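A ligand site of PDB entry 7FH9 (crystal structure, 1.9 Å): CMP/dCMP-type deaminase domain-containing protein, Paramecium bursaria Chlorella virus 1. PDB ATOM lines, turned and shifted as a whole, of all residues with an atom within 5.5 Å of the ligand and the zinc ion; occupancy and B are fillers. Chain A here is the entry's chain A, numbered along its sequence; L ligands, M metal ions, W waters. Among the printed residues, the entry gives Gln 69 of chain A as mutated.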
ATOM      1  N   ASP A  21      -5.384 -21.327  21.972  1.00  0.00           N
ATOM      2  CA  ASP A  21      -5.318 -22.779  22.144  1.00  0.00           C
ATOM      3  C   ASP A  21      -4.039 -23.310  21.504  1.00  0.00           C
ATOM      4  O   ASP A  21      -3.774 -23.025  20.330  1.00  0.00           O
ATOM      5  CB  ASP A  21      -6.539 -23.455  21.518  1.00  0.00           C
ATOM      6  CG  ASP A  21      -6.617 -24.936  21.858  1.00  0.00           C
ATOM      7  OD1 ASP A  21      -5.667 -25.679  21.529  1.00  0.00           O
ATOM      8  OD2 ASP A  21      -7.632 -25.383  22.440  1.00  0.00           O
ATOM      9  N   ASN A  23      -3.153 -26.319  20.587  1.00  0.00           N
ATOM     10  CA  ASN A  23      -3.339 -27.426  19.656  1.00  0.00           C
ATOM     11  C   ASN A  23      -4.201 -27.067  18.449  1.00  0.00           C
ATOM     12  O   ASN A  23      -3.804 -27.325  17.320  1.00  0.00           O
ATOM     13  CB  ASN A  23      -3.971 -28.626  20.380  1.00  0.00           C
ATOM     14  CG  ASN A  23      -3.083 -29.187  21.471  1.00  0.00           C
ATOM     15  OD1 ASN A  23      -1.855 -29.111  21.398  1.00  0.00           O
ATOM     16  ND2 ASN A  23      -3.706 -29.758  22.497  1.00  0.00           N
ATOM     17  N   THR A  24      -5.391 -26.486  18.671  1.00  0.00           N
ATOM     18  CA  THR A  24      -6.366 -26.295  17.614  1.00  0.00           C
ATOM     19  C   THR A  24      -6.993 -24.919  17.757  1.00  0.00           C
ATOM     20  O   THR A  24      -7.634 -24.626  18.764  1.00  0.00           O
ATOM     21  CB  THR A  24      -7.451 -27.376  17.660  1.00  0.00           C
ATOM     22  OG1 THR A  24      -6.861 -28.670  17.502  1.00  0.00           O
ATOM     23  CG2 THR A  24      -8.504 -27.162  16.594  1.00  0.00           C
ATOM     24  N   VAL A  26      -9.696 -22.124  16.299  1.00  0.00           N
ATOM     25  CA  VAL A  26     -10.984 -22.130  15.600  1.00  0.00           C
ATOM     26  C   VAL A  26     -11.548 -20.715  15.600  1.00  0.00           C
ATOM     27  O   VAL A  26     -11.471 -20.016  16.613  1.00  0.00           O
ATOM     28  CB  VAL A  26     -11.995 -23.090  16.288  1.00  0.00           C
ATOM     29  CG1 VAL A  26     -13.272 -23.217  15.482  1.00  0.00           C
ATOM     30  CG2 VAL A  26     -11.367 -24.457  16.535  1.00  0.00           C
ATOM     31  N   ASN A  43     -12.173 -19.742  19.666  1.00  0.00           N
ATOM     32  CA  ASN A  43     -12.159 -20.542  20.885  1.00  0.00           C
ATOM     33  C   ASN A  43     -11.213 -19.926  21.906  1.00  0.00           C
ATOM     34  O   ASN A  43     -10.151 -19.409  21.561  1.00  0.00           O
ATOM     35  CB  ASN A  43     -11.789 -22.014  20.601  1.00  0.00           C
ATOM     36  CG  ASN A  43     -10.449 -22.194  19.889  1.00  0.00           C
ATOM     37  OD1 ASN A  43     -10.030 -21.374  19.068  1.00  0.00           O
ATOM     38  ND2 ASN A  43      -9.771 -23.301  20.197  1.00  0.00           N
ATOM     39  N   TRP A  56      -4.722 -24.179  30.036  1.00  0.00           N
ATOM     40  CA  TRP A  56      -4.806 -24.446  28.603  1.00  0.00           C
ATOM     41  C   TRP A  56      -4.327 -25.858  28.226  1.00  0.00           C
ATOM     42  O   TRP A  56      -4.430 -26.230  27.056  1.00  0.00           O
ATOM     43  CB  TRP A  56      -4.017 -23.392  27.801  1.00  0.00           C
ATOM     44  CG  TRP A  56      -4.852 -22.207  27.354  1.00  0.00           C
ATOM     45  CD1 TRP A  56      -4.714 -20.905  27.748  1.00  0.00           C
ATOM     46  CD2 TRP A  56      -5.938 -22.233  26.430  1.00  0.00           C
ATOM     47  NE1 TRP A  56      -5.641 -20.113  27.112  1.00  0.00           N
ATOM     48  CE2 TRP A  56      -6.419 -20.902  26.308  1.00  0.00           C
ATOM     49  CE3 TRP A  56      -6.557 -23.244  25.691  1.00  0.00           C
ATOM     50  CZ2 TRP A  56      -7.475 -20.572  25.477  1.00  0.00           C
ATOM     51  CZ3 TRP A  56      -7.632 -22.913  24.873  1.00  0.00           C
ATOM     52  CH2 TRP A  56      -8.080 -21.579  24.766  1.00  0.00           C
ATOM     53  N   LYS A  58      -4.535 -30.065  28.238  1.00  0.00           N
ATOM     54  CA  LYS A  58      -5.596 -31.079  28.209  1.00  0.00           C
ATOM     55  C   LYS A  58      -5.391 -32.037  29.358  1.00  0.00           C
ATOM     56  O   LYS A  58      -4.256 -32.412  29.641  1.00  0.00           O
ATOM     57  CB  LYS A  58      -5.597 -31.858  26.892  1.00  0.00           C
ATOM     58  CG  LYS A  58      -5.587 -31.033  25.645  1.00  0.00           C
ATOM     59  CD  LYS A  58      -6.320 -31.766  24.531  1.00  0.00           C
ATOM     60  CE  LYS A  58      -5.544 -32.945  24.013  1.00  0.00           C
ATOM     61  NZ  LYS A  58      -4.534 -32.507  23.004  1.00  0.00           N
ATOM     62  N   LYS A  61      -8.358 -27.825  30.078  1.00  0.00           N
ATOM     63  CA  LYS A  61      -8.918 -26.705  29.323  1.00  0.00           C
ATOM     64  C   LYS A  61     -10.396 -26.888  29.018  1.00  0.00           C
ATOM     65  O   LYS A  61     -11.123 -25.901  28.844  1.00  0.00           O
ATOM     66  CB  LYS A  61      -8.149 -26.462  28.027  1.00  0.00           C
ATOM     67  CG  LYS A  61      -8.333 -27.537  26.959  1.00  0.00           C
ATOM     68  CD  LYS A  61      -7.521 -27.178  25.707  1.00  0.00           C
ATOM     69  CE  LYS A  61      -7.637 -28.258  24.634  1.00  0.00           C
ATOM     70  NZ  LYS A  61      -6.609 -28.061  23.559  1.00  0.00           N
ATOM     71  N   TYR A  62     -10.887 -28.124  28.947  1.00  0.00           N
ATOM     72  CA  TYR A  62     -12.300 -28.303  28.594  1.00  0.00           C
ATOM     73  C   TYR A  62     -13.243 -27.797  29.682  1.00  0.00           C
ATOM     74  O   TYR A  62     -14.397 -27.490  29.381  1.00  0.00           O
ATOM     75  CB  TYR A  62     -12.591 -29.766  28.257  1.00  0.00           C
ATOM     76  CG  TYR A  62     -11.736 -30.277  27.114  1.00  0.00           C
ATOM     77  CD1 TYR A  62     -11.849 -29.755  25.826  1.00  0.00           C
ATOM     78  CD2 TYR A  62     -10.807 -31.283  27.327  1.00  0.00           C
ATOM     79  CE1 TYR A  62     -11.053 -30.218  24.794  1.00  0.00           C
ATOM     80  CE2 TYR A  62     -10.014 -31.763  26.305  1.00  0.00           C
ATOM     81  CZ  TYR A  62     -10.142 -31.220  25.043  1.00  0.00           C
ATOM     82  OH  TYR A  62      -9.339 -31.717  24.036  1.00  0.00           O
ATOM     83  N   VAL A  65     -12.996 -23.746  28.411  1.00  0.00           N
ATOM     84  CA  VAL A  65     -12.955 -23.210  27.047  1.00  0.00           C
ATOM     85  C   VAL A  65     -14.366 -23.037  26.491  1.00  0.00           C
ATOM     86  O   VAL A  65     -15.304 -23.769  26.843  1.00  0.00           O
ATOM     87  CB  VAL A  65     -12.103 -24.119  26.130  1.00  0.00           C
ATOM     88  CG1 VAL A  65     -12.793 -25.434  25.869  1.00  0.00           C
ATOM     89  CG2 VAL A  65     -11.795 -23.398  24.803  1.00  0.00           C
ATOM     90  N   VAL A  66     -14.510 -22.026  25.630  1.00  0.00           N
ATOM     91  CA  VAL A  66     -15.742 -21.727  24.899  1.00  0.00           C
ATOM     92  C   VAL A  66     -15.475 -21.977  23.422  1.00  0.00           C
ATOM     93  O   VAL A  66     -14.451 -21.511  22.891  1.00  0.00           O
ATOM     94  CB  VAL A  66     -16.198 -20.275  25.122  1.00  0.00           C
ATOM     95  CG1 VAL A  66     -17.494 -19.971  24.301  1.00  0.00           C
ATOM     96  CG2 VAL A  66     -16.404 -19.973  26.623  1.00  0.00           C
ATOM     97  N   HIS A  67     -16.383 -22.688  22.751  1.00  0.00           N
ATOM     98  CA  HIS A  67     -16.253 -22.916  21.320  1.00  0.00           C
ATOM     99  C   HIS A  67     -16.387 -21.618  20.533  1.00  0.00           C
ATOM    100  O   HIS A  67     -17.077 -20.688  20.955  1.00  0.00           O
ATOM    101  CB  HIS A  67     -17.313 -23.931  20.840  1.00  0.00           C
ATOM    102  CG  HIS A  67     -17.011 -25.345  21.223  1.00  0.00           C
ATOM    103  ND1 HIS A  67     -17.762 -26.413  20.764  1.00  0.00           N
ATOM    104  CD2 HIS A  67     -16.047 -25.872  22.018  1.00  0.00           C
ATOM    105  CE1 HIS A  67     -17.271 -27.538  21.265  1.00  0.00           C
ATOM    106  NE2 HIS A  67     -16.226 -27.233  22.026  1.00  0.00           N
ATOM    107  N   ALA A  68     -15.748 -21.579  19.363  1.00  0.00           N
ATOM    108  CA  ALA A  68     -15.755 -20.353  18.562  1.00  0.00           C
ATOM    109  C   ALA A  68     -17.175 -19.939  18.171  1.00  0.00           C
ATOM    110  O   ALA A  68     -17.511 -18.747  18.200  1.00  0.00           O
ATOM    111  CB  ALA A  68     -14.902 -20.551  17.305  1.00  0.00           C
ATOM    112  N   GLN A  69     -18.017 -20.896  17.760  1.00  0.00           N
ATOM    113  CA  GLN A  69     -19.326 -20.502  17.261  1.00  0.00           C
ATOM    114  C   GLN A  69     -20.235 -20.051  18.405  1.00  0.00           C
ATOM    115  O   GLN A  69     -20.918 -19.026  18.286  1.00  0.00           O
ATOM    116  CB  GLN A  69     -19.930 -21.638  16.428  1.00  0.00           C
ATOM    117  CG  GLN A  69     -19.096 -21.817  15.136  1.00  0.00           C
ATOM    118  CD  GLN A  69     -19.499 -22.977  14.239  1.00  0.00           C
ATOM    119  OE1 GLN A  69     -20.502 -22.908  13.526  1.00  0.00           O
ATOM    120  NE2 GLN A  69     -18.700 -24.035  14.252  1.00  0.00           N
ATOM    121  N   LEU A  92     -14.612 -24.722  11.364  1.00  0.00           N
ATOM    122  CA  LEU A  92     -14.889 -26.087  11.800  1.00  0.00           C
ATOM    123  C   LEU A  92     -16.390 -26.283  11.860  1.00  0.00           C
ATOM    124  O   LEU A  92     -17.088 -25.430  12.406  1.00  0.00           O
ATOM    125  CB  LEU A  92     -14.240 -26.343  13.172  1.00  0.00           C
ATOM    126  CG  LEU A  92     -14.410 -27.696  13.831  1.00  0.00           C
ATOM    127  CD1 LEU A  92     -13.745 -28.773  12.984  1.00  0.00           C
ATOM    128  CD2 LEU A  92     -13.790 -27.642  15.242  1.00  0.00           C
ATOM    129  N   PHE A  93     -16.889 -27.392  11.309  1.00  0.00           N
ATOM    130  CA  PHE A  93     -18.328 -27.646  11.355  1.00  0.00           C
ATOM    131  C   PHE A  93     -18.785 -27.730  12.815  1.00  0.00           C
ATOM    132  O   PHE A  93     -18.103 -28.361  13.637  1.00  0.00           O
ATOM    133  CB  PHE A  93     -18.670 -28.946  10.617  1.00  0.00           C
ATOM    134  CG  PHE A  93     -20.148 -29.211  10.484  1.00  0.00           C
ATOM    135  CD1 PHE A  93     -20.861 -29.820  11.514  1.00  0.00           C
ATOM    136  CD2 PHE A  93     -20.825 -28.862   9.322  1.00  0.00           C
ATOM    137  CE1 PHE A  93     -22.215 -30.060  11.386  1.00  0.00           C
ATOM    138  CE2 PHE A  93     -22.193 -29.110   9.196  1.00  0.00           C
ATOM    139  CZ  PHE A  93     -22.886 -29.707  10.232  1.00  0.00           C
ATOM    140  N   PRO A  94     -19.926 -27.133  13.153  1.00  0.00           N
ATOM    141  CA  PRO A  94     -20.302 -27.013  14.561  1.00  0.00           C
ATOM    142  C   PRO A  94     -20.622 -28.338  15.232  1.00  0.00           C
ATOM    143  O   PRO A  94     -21.177 -29.259  14.615  1.00  0.00           O
ATOM    144  CB  PRO A  94     -21.548 -26.118  14.521  1.00  0.00           C
ATOM    145  CG  PRO A  94     -22.101 -26.313  13.120  1.00  0.00           C
ATOM    146  CD  PRO A  94     -20.878 -26.444  12.256  1.00  0.00           C
ATOM    147  N   CYS A  95     -20.295 -28.412  16.516  1.00  0.00           N
ATOM    148  CA  CYS A  95     -20.731 -29.529  17.338  1.00  0.00           C
ATOM    149  C   CYS A  95     -22.239 -29.460  17.563  1.00  0.00           C
ATOM    150  O   CYS A  95     -22.906 -28.470  17.226  1.00  0.00           O
ATOM    151  CB  CYS A  95     -20.001 -29.538  18.689  1.00  0.00           C
ATOM    152  SG  CYS A  95     -20.577 -28.251  19.871  1.00  0.00           S
ATOM    153  N   GLU A  97     -24.003 -29.028  20.284  1.00  0.00           N
ATOM    154  CA  GLU A  97     -24.513 -27.950  21.127  1.00  0.00           C
ATOM    155  C   GLU A  97     -24.449 -26.602  20.426  1.00  0.00           C
ATOM    156  O   GLU A  97     -25.385 -25.800  20.532  1.00  0.00           O
ATOM    157  CB  GLU A  97     -23.755 -27.914  22.462  1.00  0.00           C
ATOM    158  CG  GLU A  97     -23.717 -29.273  23.162  1.00  0.00           C
ATOM    159  CD  GLU A  97     -25.112 -29.787  23.569  1.00  0.00           C
ATOM    160  OE1 GLU A  97     -26.056 -28.979  23.571  1.00  0.00           O
ATOM    161  OE2 GLU A  97     -25.239 -30.985  23.883  1.00  0.00           O
ATOM    162  N   CYS A  98     -23.359 -26.325  19.718  1.00  0.00           N
ATOM    163  CA  CYS A  98     -23.283 -25.074  18.965  1.00  0.00           C
ATOM    164  C   CYS A  98     -24.324 -25.019  17.864  1.00  0.00           C
ATOM    165  O   CYS A  98     -24.839 -23.939  17.547  1.00  0.00           O
ATOM    166  CB  CYS A  98     -21.878 -24.882  18.380  1.00  0.00           C
ATOM    167  SG  CYS A  98     -20.592 -24.408  19.615  1.00  0.00           S
ATOM    168  N   TRP A 121     -17.315 -38.830  15.654  1.00  0.00           N
ATOM    169  CA  TRP A 121     -18.165 -37.648  15.497  1.00  0.00           C
ATOM    170  C   TRP A 121     -19.389 -37.892  14.620  1.00  0.00           C
ATOM    171  O   TRP A 121     -20.170 -36.964  14.394  1.00  0.00           O
ATOM    172  CB  TRP A 121     -17.363 -36.485  14.923  1.00  0.00           C
ATOM    173  CG  TRP A 121     -16.474 -35.814  15.917  1.00  0.00           C
ATOM    174  CD1 TRP A 121     -15.153 -36.091  16.152  1.00  0.00           C
ATOM    175  CD2 TRP A 121     -16.826 -34.767  16.822  1.00  0.00           C
ATOM    176  NE1 TRP A 121     -14.671 -35.271  17.149  1.00  0.00           N
ATOM    177  CE2 TRP A 121     -15.676 -34.440  17.577  1.00  0.00           C
ATOM    178  CE3 TRP A 121     -18.010 -34.052  17.066  1.00  0.00           C
ATOM    179  CZ2 TRP A 121     -15.674 -33.448  18.550  1.00  0.00           C
ATOM    180  CZ3 TRP A 121     -18.002 -33.073  18.040  1.00  0.00           C
ATOM    181  CH2 TRP A 121     -16.844 -32.778  18.767  1.00  0.00           C
HETATM  182  P1  LIG L   1      -7.985 -30.186  21.015  1.00  0.00           P
HETATM  183  O1  LIG L   1      -7.750 -30.198  19.521  1.00  0.00           O
HETATM  184  O2  LIG L   1      -6.688 -30.203  21.811  1.00  0.00           O
HETATM  185  O3  LIG L   1      -8.973 -31.235  21.479  1.00  0.00           O
HETATM  186  O4  LIG L   1      -8.676 -28.764  21.339  1.00  0.00           O
HETATM  187  C1  LIG L   1      -9.814 -28.342  20.547  1.00  0.00           C
HETATM  188  C2  LIG L   1     -10.040 -26.863  20.739  1.00  0.00           C
HETATM  189  O5  LIG L   1     -11.009 -26.384  19.773  1.00  0.00           O
HETATM  190  C3  LIG L   1     -10.581 -26.464  22.111  1.00  0.00           C
HETATM  191  O6  LIG L   1     -10.087 -25.187  22.490  1.00  0.00           O
HETATM  192  C4  LIG L   1     -12.084 -26.419  21.869  1.00  0.00           C
HETATM  193  C5  LIG L   1     -12.178 -25.914  20.431  1.00  0.00           C
HETATM  194  N1  LIG L   1     -13.345 -26.424  19.685  1.00  0.00           N
HETATM  195  C6  LIG L   1     -14.209 -25.510  19.129  1.00  0.00           C
HETATM  196  O7  LIG L   1     -14.043 -24.295  19.228  1.00  0.00           O
HETATM  197  N2  LIG L   1     -15.272 -26.045  18.454  1.00  0.00           N
HETATM  198  C7  LIG L   1     -15.540 -27.394  18.281  1.00  0.00           C
HETATM  199  O8  LIG L   1     -16.547 -27.736  17.643  1.00  0.00           O
HETATM  200  C8  LIG L   1     -14.601 -28.304  18.888  1.00  0.00           C
HETATM  201  C9  LIG L   1     -14.822 -29.777  18.745  1.00  0.00           C
HETATM  202  C10 LIG L   1     -13.559 -27.780  19.557  1.00  0.00           C
HETATM  203 ZN    ZN M   1     -19.412 -26.321  19.611  1.00  0.00          ZN
HETATM  204  O   HOH W   1     -18.562 -26.309  17.685  1.00  0.00           O
HETATM  205  O   HOH W   2     -16.960 -23.831  16.977  1.00  0.00           O
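SG of Cys 95 lies close to N of Glu 97.
The backbone NH (N) of Thr 24 sits at hydrogen-bond distance from the side-chain carboxylate (OD1) of Asp 21.
The side-chain amino group (NZ) of Lys 61 lies within salt-bridge range of the side-chain carboxylate (OD2) of Asp 21 (3.1 Å).
OD1 of Asp 21 sits at hydrogen-bond distance from N of Asn 23 (2.8 Å).
O of Thr 24 lies within hydrogen-bond range of ND2 of Asn 43, at 2.9 Å.
The side-chain amide oxygen (OD1) of Asn 43 sits at hydrogen-bond distance from the backbone NH (N) of Val 26 (2.9 Å).
NZ of Lys 58 lies close to ND2 of Asn 23 (2.9 Å).
NE2 of Gln 69 is in hydrogen-bond range of O of Leu 92, 2.8 Å away.
N2 of the ligand sits close to ND1 of His 67 (3.4 Å).
An oxygen (O6) of the ligand sits at hydrogen-bond distance from the side-chain carboxylate (OD2) of Asp 21, 2.5 Å away.
OH of Tyr 62 sits at hydrogen-bond distance from O3 of the ligand.
An oxygen (O1) of the ligand is in hydrogen-bond range of the side-chain hydroxyl (OG1) of Thr 24, 2.7 Å away.
An oxygen (O2) of the ligand lies within salt-bridge range of the side-chain amino group (NZ) of Lys 61 (2.8 Å).
An oxygen (O6) of the ligand lies within hydrogen-bond range of the side-chain amide nitrogen (ND2) of Asn 43 (3.0 Å).
ND2 of Asn 23 lies within hydrogen-bond range of O2 of the ligand, 3.1 Å away.
O2 of the ligand lies within salt-bridge range of NZ of Lys 58 (3.4 Å).
An oxygen (O7) of the ligand sits at hydrogen-bond distance from the backbone NH of Ala 68 (3.2 Å).
Water W1 bridges O8 of the ligand and N of Cys 95.
The zinc ion is bound by a ring nitrogen (ND1) of His 67 (2.0 Å), water W1 (2.1 Å), the side-chain sulfur of Cys 98 (2.2 Å) and the side-chain sulfur of Cys 95 (2.3 Å).
Merely in contact with the ligand: Val 26, Val 65, Leu 92 and Trp 121.
Hydrophobic or aromatic side chains within 4 Å of the ligand: Val 26, Tyr 62, Val 65, His 67, Leu 92 and Trp 121.
Within 4 Å of the ligand: Asp 21, Asn 23, Thr 24, Val 26, Asn 43, Lys 58, Lys 61, Tyr 62, Val 65, His 67, Ala 68, Leu 92, Cys 95 and Trp 121.
Along chain A the residues within 4 Å of the ligand span positions 21 to 121.
The nearest printed residue that does not touch the ligand is Trp 56 (4.1 Å).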
